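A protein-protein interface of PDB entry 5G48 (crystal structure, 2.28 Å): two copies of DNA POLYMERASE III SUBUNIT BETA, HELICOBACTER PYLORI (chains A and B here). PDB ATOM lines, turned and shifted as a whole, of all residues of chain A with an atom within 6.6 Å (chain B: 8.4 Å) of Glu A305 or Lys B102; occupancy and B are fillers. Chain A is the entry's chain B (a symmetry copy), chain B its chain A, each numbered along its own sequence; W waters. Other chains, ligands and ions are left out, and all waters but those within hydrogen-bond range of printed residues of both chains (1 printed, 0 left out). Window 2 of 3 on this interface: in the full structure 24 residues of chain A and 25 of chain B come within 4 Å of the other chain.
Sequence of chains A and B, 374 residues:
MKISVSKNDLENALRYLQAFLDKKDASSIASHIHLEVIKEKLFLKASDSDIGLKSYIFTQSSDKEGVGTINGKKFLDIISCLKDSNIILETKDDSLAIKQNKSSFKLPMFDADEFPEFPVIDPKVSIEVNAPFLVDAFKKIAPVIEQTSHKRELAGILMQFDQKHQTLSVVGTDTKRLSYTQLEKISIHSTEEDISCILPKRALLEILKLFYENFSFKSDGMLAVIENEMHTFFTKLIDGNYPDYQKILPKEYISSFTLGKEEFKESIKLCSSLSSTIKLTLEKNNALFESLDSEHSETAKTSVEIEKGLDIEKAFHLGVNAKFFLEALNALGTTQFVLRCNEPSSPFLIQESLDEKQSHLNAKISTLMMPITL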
ATOM      1  N   GLU A 263      18.738  32.208  -7.142  1.00  0.00           N
ATOM      2  CA  GLU A 263      18.219  31.406  -6.034  1.00  0.00           C
ATOM      3  C   GLU A 263      16.830  30.841  -6.333  1.00  0.00           C
ATOM      4  O   GLU A 263      16.574  29.666  -6.058  1.00  0.00           O
ATOM      5  CB  GLU A 263      18.193  32.208  -4.726  1.00  0.00           C
ATOM      6  CG  GLU A 263      19.531  32.254  -4.005  1.00  0.00           C
ATOM      7  CD  GLU A 263      19.420  32.802  -2.595  1.00  0.00           C
ATOM      8  OE1 GLU A 263      18.499  33.601  -2.325  1.00  0.00           O
ATOM      9  OE2 GLU A 263      20.260  32.446  -1.751  1.00  0.00           O
ATOM     10  N   ASN A 285      11.430  36.393   6.240  1.00  0.00           N
ATOM     11  CA  ASN A 285      12.847  36.107   5.931  1.00  0.00           C
ATOM     12  C   ASN A 285      13.113  34.764   5.223  1.00  0.00           C
ATOM     13  O   ASN A 285      14.255  34.284   5.224  1.00  0.00           O
ATOM     14  CB  ASN A 285      13.682  36.145   7.222  1.00  0.00           C
ATOM     15  CG  ASN A 285      13.724  37.516   7.859  1.00  0.00           C
ATOM     16  OD1 ASN A 285      13.384  37.668   9.029  1.00  0.00           O
ATOM     17  ND2 ASN A 285      14.166  38.516   7.101  1.00  0.00           N
ATOM     18  N   ASN A 286      12.090  34.162   4.615  1.00  0.00           N
ATOM     19  CA  ASN A 286      12.260  32.897   3.890  1.00  0.00           C
ATOM     20  C   ASN A 286      11.366  32.775   2.669  1.00  0.00           C
ATOM     21  O   ASN A 286      10.297  33.379   2.595  1.00  0.00           O
ATOM     22  CB  ASN A 286      12.002  31.693   4.810  1.00  0.00           C
ATOM     23  CG  ASN A 286      13.141  31.435   5.772  1.00  0.00           C
ATOM     24  OD1 ASN A 286      14.117  30.766   5.431  1.00  0.00           O
ATOM     25  ND2 ASN A 286      13.027  31.967   6.984  1.00  0.00           N
ATOM     26  N   ALA A 287      11.833  31.981   1.713  1.00  0.00           N
ATOM     27  CA  ALA A 287      11.034  31.545   0.581  1.00  0.00           C
ATOM     28  C   ALA A 287      11.073  30.031   0.591  1.00  0.00           C
ATOM     29  O   ALA A 287      12.151  29.454   0.471  1.00  0.00           O
ATOM     30  CB  ALA A 287      11.613  32.081  -0.716  1.00  0.00           C
ATOM     31  N   LYS A 301      11.000  19.444  -1.565  1.00  0.00           N
ATOM     32  CA  LYS A 301      10.904  20.684  -0.804  1.00  0.00           C
ATOM     33  C   LYS A 301      12.267  21.347  -0.728  1.00  0.00           C
ATOM     34  O   LYS A 301      13.291  20.666  -0.607  1.00  0.00           O
ATOM     35  CB  LYS A 301      10.436  20.401   0.626  1.00  0.00           C
ATOM     36  CG  LYS A 301       9.121  19.638   0.741  1.00  0.00           C
ATOM     37  CD  LYS A 301       8.826  19.232   2.180  1.00  0.00           C
ATOM     38  CE  LYS A 301       8.418  20.420   3.043  1.00  0.00           C
ATOM     39  NZ  LYS A 301       8.274  20.048   4.477  1.00  0.00           N
ATOM     40  N   THR A 302      12.282  22.673  -0.805  1.00  0.00           N
ATOM     41  CA  THR A 302      13.460  23.434  -0.425  1.00  0.00           C
ATOM     42  C   THR A 302      13.070  24.817   0.050  1.00  0.00           C
ATOM     43  O   THR A 302      11.930  25.246  -0.119  1.00  0.00           O
ATOM     44  CB  THR A 302      14.508  23.523  -1.557  1.00  0.00           C
ATOM     45  OG1 THR A 302      15.709  24.122  -1.052  1.00  0.00           O
ATOM     46  CG2 THR A 302      14.001  24.335  -2.736  1.00  0.00           C
ATOM     47  N   SER A 303      14.031  25.488   0.670  1.00  0.00           N
ATOM     48  CA  SER A 303      13.873  26.868   1.090  1.00  0.00           C
ATOM     49  C   SER A 303      15.161  27.652   0.865  1.00  0.00           C
ATOM     50  O   SER A 303      16.217  27.084   0.572  1.00  0.00           O
ATOM     51  CB  SER A 303      13.430  26.960   2.563  1.00  0.00           C
ATOM     52  OG  SER A 303      14.479  26.635   3.462  1.00  0.00           O
ATOM     53  N   VAL A 304      15.037  28.962   1.013  1.00  0.00           N
ATOM     54  CA  VAL A 304      16.122  29.907   0.824  1.00  0.00           C
ATOM     55  C   VAL A 304      15.885  31.058   1.802  1.00  0.00           C
ATOM     56  O   VAL A 304      14.744  31.469   2.014  1.00  0.00           O
ATOM     57  CB  VAL A 304      16.151  30.374  -0.660  1.00  0.00           C
ATOM     58  CG1 VAL A 304      16.458  31.857  -0.812  1.00  0.00           C
ATOM     59  CG2 VAL A 304      17.128  29.526  -1.474  1.00  0.00           C
ATOM     60  N   GLU A 305      16.958  31.566   2.400  1.00  0.00           N
ATOM     61  CA  GLU A 305      16.862  32.695   3.320  1.00  0.00           C
ATOM     62  C   GLU A 305      16.805  34.013   2.545  1.00  0.00           C
ATOM     63  O   GLU A 305      17.555  34.208   1.588  1.00  0.00           O
ATOM     64  CB  GLU A 305      18.052  32.706   4.281  1.00  0.00           C
ATOM     65  CG  GLU A 305      18.033  33.849   5.287  1.00  0.00           C
ATOM     66  CD  GLU A 305      19.066  33.709   6.396  1.00  0.00           C
ATOM     67  OE1 GLU A 305      19.841  32.721   6.414  1.00  0.00           O
ATOM     68  OE2 GLU A 305      19.103  34.612   7.256  1.00  0.00           O
ATOM     69  N   ILE A 306      15.912  34.901   2.975  1.00  0.00           N
ATOM     70  CA  ILE A 306      15.851  36.282   2.509  1.00  0.00           C
ATOM     71  C   ILE A 306      16.367  37.153   3.655  1.00  0.00           C
ATOM     72  O   ILE A 306      15.728  37.246   4.704  1.00  0.00           O
ATOM     73  CB  ILE A 306      14.409  36.694   2.135  1.00  0.00           C
ATOM     74  CG1 ILE A 306      13.850  35.775   1.042  1.00  0.00           C
ATOM     75  CG2 ILE A 306      14.364  38.144   1.667  1.00  0.00           C
ATOM     76  CD1 ILE A 306      12.339  35.737   0.999  1.00  0.00           C
ATOM     77  N   GLU A 307      17.533  37.764   3.464  1.00  0.00           N
ATOM     78  CA  GLU A 307      18.144  38.611   4.497  1.00  0.00           C
ATOM     79  C   GLU A 307      17.394  39.916   4.667  1.00  0.00           C
ATOM     80  O   GLU A 307      17.029  40.285   5.781  1.00  0.00           O
ATOM     81  CB  GLU A 307      19.591  38.937   4.150  1.00  0.00           C
ATOM     82  CG  GLU A 307      20.514  37.739   4.136  1.00  0.00           C
ATOM     83  CD  GLU A 307      21.959  38.155   4.197  1.00  0.00           C
ATOM     84  OE1 GLU A 307      22.382  38.659   5.259  1.00  0.00           O
ATOM     85  OE2 GLU A 307      22.659  37.998   3.178  1.00  0.00           O
ATOM     86  N   LEU B  82      21.146  19.855  -7.233  1.00  0.00           N
ATOM     87  CA  LEU B  82      21.573  20.213  -5.871  1.00  0.00           C
ATOM     88  C   LEU B  82      22.951  20.896  -5.843  1.00  0.00           C
ATOM     89  O   LEU B  82      23.628  20.992  -6.858  1.00  0.00           O
ATOM     90  CB  LEU B  82      21.549  18.965  -4.971  1.00  0.00           C
ATOM     91  CG  LEU B  82      20.160  18.409  -4.624  1.00  0.00           C
ATOM     92  CD1 LEU B  82      20.263  17.043  -3.964  1.00  0.00           C
ATOM     93  CD2 LEU B  82      19.396  19.365  -3.723  1.00  0.00           C
ATOM     94  N   LYS B  83      23.329  21.388  -4.666  1.00  0.00           N
ATOM     95  CA  LYS B  83      24.615  22.061  -4.437  1.00  0.00           C
ATOM     96  C   LYS B  83      25.755  21.060  -4.254  1.00  0.00           C
ATOM     97  O   LYS B  83      25.509  19.863  -4.112  1.00  0.00           O
ATOM     98  CB  LYS B  83      24.511  22.950  -3.192  1.00  0.00           C
ATOM     99  CG  LYS B  83      23.622  24.170  -3.379  1.00  0.00           C
ATOM    100  CD  LYS B  83      23.008  24.653  -2.068  1.00  0.00           C
ATOM    101  CE  LYS B  83      22.904  26.172  -1.982  1.00  0.00           C
ATOM    102  NZ  LYS B  83      22.412  26.825  -3.228  1.00  0.00           N
ATOM    103  N   SER B  85      27.658  19.910  -1.850  1.00  0.00           N
ATOM    104  CA  SER B  85      27.908  19.502  -0.464  1.00  0.00           C
ATOM    105  C   SER B  85      27.247  18.147  -0.237  1.00  0.00           C
ATOM    106  O   SER B  85      26.506  17.671  -1.098  1.00  0.00           O
ATOM    107  CB  SER B  85      27.385  20.546   0.533  1.00  0.00           C
ATOM    108  OG  SER B  85      25.970  20.574   0.585  1.00  0.00           O
ATOM    109  N   ILE B  98      15.900  11.899   0.604  1.00  0.00           N
ATOM    110  CA  ILE B  98      17.148  12.544   0.187  1.00  0.00           C
ATOM    111  C   ILE B  98      17.180  13.903   0.870  1.00  0.00           C
ATOM    112  O   ILE B  98      16.209  14.638   0.776  1.00  0.00           O
ATOM    113  CB  ILE B  98      17.213  12.755  -1.343  1.00  0.00           C
ATOM    114  CG1 ILE B  98      16.986  11.433  -2.088  1.00  0.00           C
ATOM    115  CG2 ILE B  98      18.558  13.357  -1.743  1.00  0.00           C
ATOM    116  CD1 ILE B  98      16.620  11.604  -3.546  1.00  0.00           C
ATOM    117  N   LYS B  99      18.280  14.230   1.553  1.00  0.00           N
ATOM    118  CA  LYS B  99      18.395  15.494   2.295  1.00  0.00           C
ATOM    119  C   LYS B  99      19.741  16.174   2.060  1.00  0.00           C
ATOM    120  O   LYS B  99      20.786  15.539   2.194  1.00  0.00           O
ATOM    121  CB  LYS B  99      18.187  15.262   3.791  1.00  0.00           C
ATOM    122  CG  LYS B  99      16.896  14.517   4.109  1.00  0.00           C
ATOM    123  CD  LYS B  99      16.419  14.699   5.546  1.00  0.00           C
ATOM    124  CE  LYS B  99      14.896  14.788   5.609  1.00  0.00           C
ATOM    125  NZ  LYS B  99      14.391  14.995   6.998  1.00  0.00           N
ATOM    126  N   GLN B 100      19.694  17.455   1.687  1.00  0.00           N
ATOM    127  CA  GLN B 100      20.877  18.320   1.582  1.00  0.00           C
ATOM    128  C   GLN B 100      20.554  19.673   2.216  1.00  0.00           C
ATOM    129  O   GLN B 100      19.997  20.559   1.556  1.00  0.00           O
ATOM    130  CB  GLN B 100      21.310  18.507   0.123  1.00  0.00           C
ATOM    131  CG  GLN B 100      22.619  19.280  -0.029  1.00  0.00           C
ATOM    132  CD  GLN B 100      22.916  19.682  -1.458  1.00  0.00           C
ATOM    133  OE1 GLN B 100      22.249  20.560  -2.020  1.00  0.00           O
ATOM    134  NE2 GLN B 100      23.935  19.064  -2.050  1.00  0.00           N
ATOM    135  N   ASN B 101      20.904  19.813   3.494  1.00  0.00           N
ATOM    136  CA  ASN B 101      20.590  20.999   4.294  1.00  0.00           C
ATOM    137  C   ASN B 101      19.094  21.387   4.188  1.00  0.00           C
ATOM    138  O   ASN B 101      18.249  20.694   4.760  1.00  0.00           O
ATOM    139  CB  ASN B 101      21.577  22.138   3.957  1.00  0.00           C
ATOM    140  CG  ASN B 101      21.412  23.366   4.854  1.00  0.00           C
ATOM    141  OD1 ASN B 101      20.783  23.310   5.911  1.00  0.00           O
ATOM    142  ND2 ASN B 101      21.996  24.482   4.432  1.00  0.00           N
ATOM    143  N   LYS B 102      18.754  22.431   3.433  1.00  0.00           N
ATOM    144  CA  LYS B 102      17.369  22.925   3.366  1.00  0.00           C
ATOM    145  C   LYS B 102      16.486  22.186   2.349  1.00  0.00           C
ATOM    146  O   LYS B 102      15.262  22.324   2.384  1.00  0.00           O
ATOM    147  CB  LYS B 102      17.360  24.430   3.079  1.00  0.00           C
ATOM    148  CG  LYS B 102      17.886  25.240   4.251  1.00  0.00           C
ATOM    149  CD  LYS B 102      18.067  26.700   3.889  1.00  0.00           C
ATOM    150  CE  LYS B 102      18.267  27.549   5.133  1.00  0.00           C
ATOM    151  NZ  LYS B 102      18.350  28.987   4.771  1.00  0.00           N
ATOM    152  N   SER B 103      17.102  21.403   1.463  1.00  0.00           N
ATOM    153  CA  SER B 103      16.371  20.647   0.451  1.00  0.00           C
ATOM    154  C   SER B 103      16.095  19.217   0.929  1.00  0.00           C
ATOM    155  O   SER B 103      16.994  18.553   1.447  1.00  0.00           O
ATOM    156  CB  SER B 103      17.170  20.631  -0.844  1.00  0.00           C
ATOM    157  OG  SER B 103      17.510  21.956  -1.237  1.00  0.00           O
ATOM    158  N   SER B 104      14.856  18.749   0.758  1.00  0.00           N
ATOM    159  CA  SER B 104      14.499  17.366   1.098  1.00  0.00           C
ATOM    160  C   SER B 104      13.477  16.766   0.133  1.00  0.00           C
ATOM    161  O   SER B 104      12.564  17.452  -0.332  1.00  0.00           O
ATOM    162  CB  SER B 104      14.003  17.264   2.545  1.00  0.00           C
ATOM    163  OG  SER B 104      12.831  18.025   2.743  1.00  0.00           O
ATOM    164  N   PHE B 105      13.655  15.480  -0.166  1.00  0.00           N
ATOM    165  CA  PHE B 105      12.864  14.771  -1.178  1.00  0.00           C
ATOM    166  C   PHE B 105      12.474  13.403  -0.655  1.00  0.00           C
ATOM    167  O   PHE B 105      13.265  12.757   0.033  1.00  0.00           O
ATOM    168  CB  PHE B 105      13.673  14.575  -2.466  1.00  0.00           C
ATOM    169  CG  PHE B 105      14.360  15.820  -2.954  1.00  0.00           C
ATOM    170  CD1 PHE B 105      15.562  16.228  -2.391  1.00  0.00           C
ATOM    171  CD2 PHE B 105      13.807  16.585  -3.971  1.00  0.00           C
ATOM    172  CE1 PHE B 105      16.197  17.378  -2.823  1.00  0.00           C
ATOM    173  CE2 PHE B 105      14.438  17.735  -4.417  1.00  0.00           C
ATOM    174  CZ  PHE B 105      15.639  18.134  -3.840  1.00  0.00           C
HETATM  175  O   HOH W   1      19.452  30.571   2.057  1.00  0.00           O
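The backbone NH of Lys A301 lies within hydrogen-bond range of the backbone carbonyl oxygen of Ser B104, 2.8 Å away. The side-chain hydroxyl (OG) of Ser B103 lies within hydrogen-bond range of the side-chain hydroxyl (OG1) of Thr A302, at 2.8 Å.
Among the printed residues, pairs that only touch across the chains: Lys A301 with Ser B103, Thr A302 with Lys B102, Ser A303 with Lys B102, Glu A305 with Lys B102 and Lys A301 with Lys B102.
Glu A263 touches none of the printed residues of chain B. Printed residues of chain B within 4 Å of Thr A302: Lys B102 and Ser B103. Glu A305 touches just one residue of chain B: Lys B102 (3.8 Å). Ile A306 touches none of the printed residues of chain B. Lys B102 touches just these residues of chain A: Lys A301, Thr A302, Ser A303 and Glu A305. Of the printed residues of chain A, Ser B103 touches Lys A301 and Thr A302. The nearest printed residue of chain B that does not touch Lys A301 is Phe B105 (4.7 Å).
Of the 11 printed residues of chain B, 3 touch a printed residue of chain A. Along chain B the printed residues that touch a printed residue of chain A span positions 102 to 104.
No position is printed for both chains. Of the 7 pairs that touch across the chains among the printed residues, none has its exchanged pair printed and touching as well.
Water W1 bridges the backbone NH of Glu A305 and the side-chain amino group of Lys B102.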
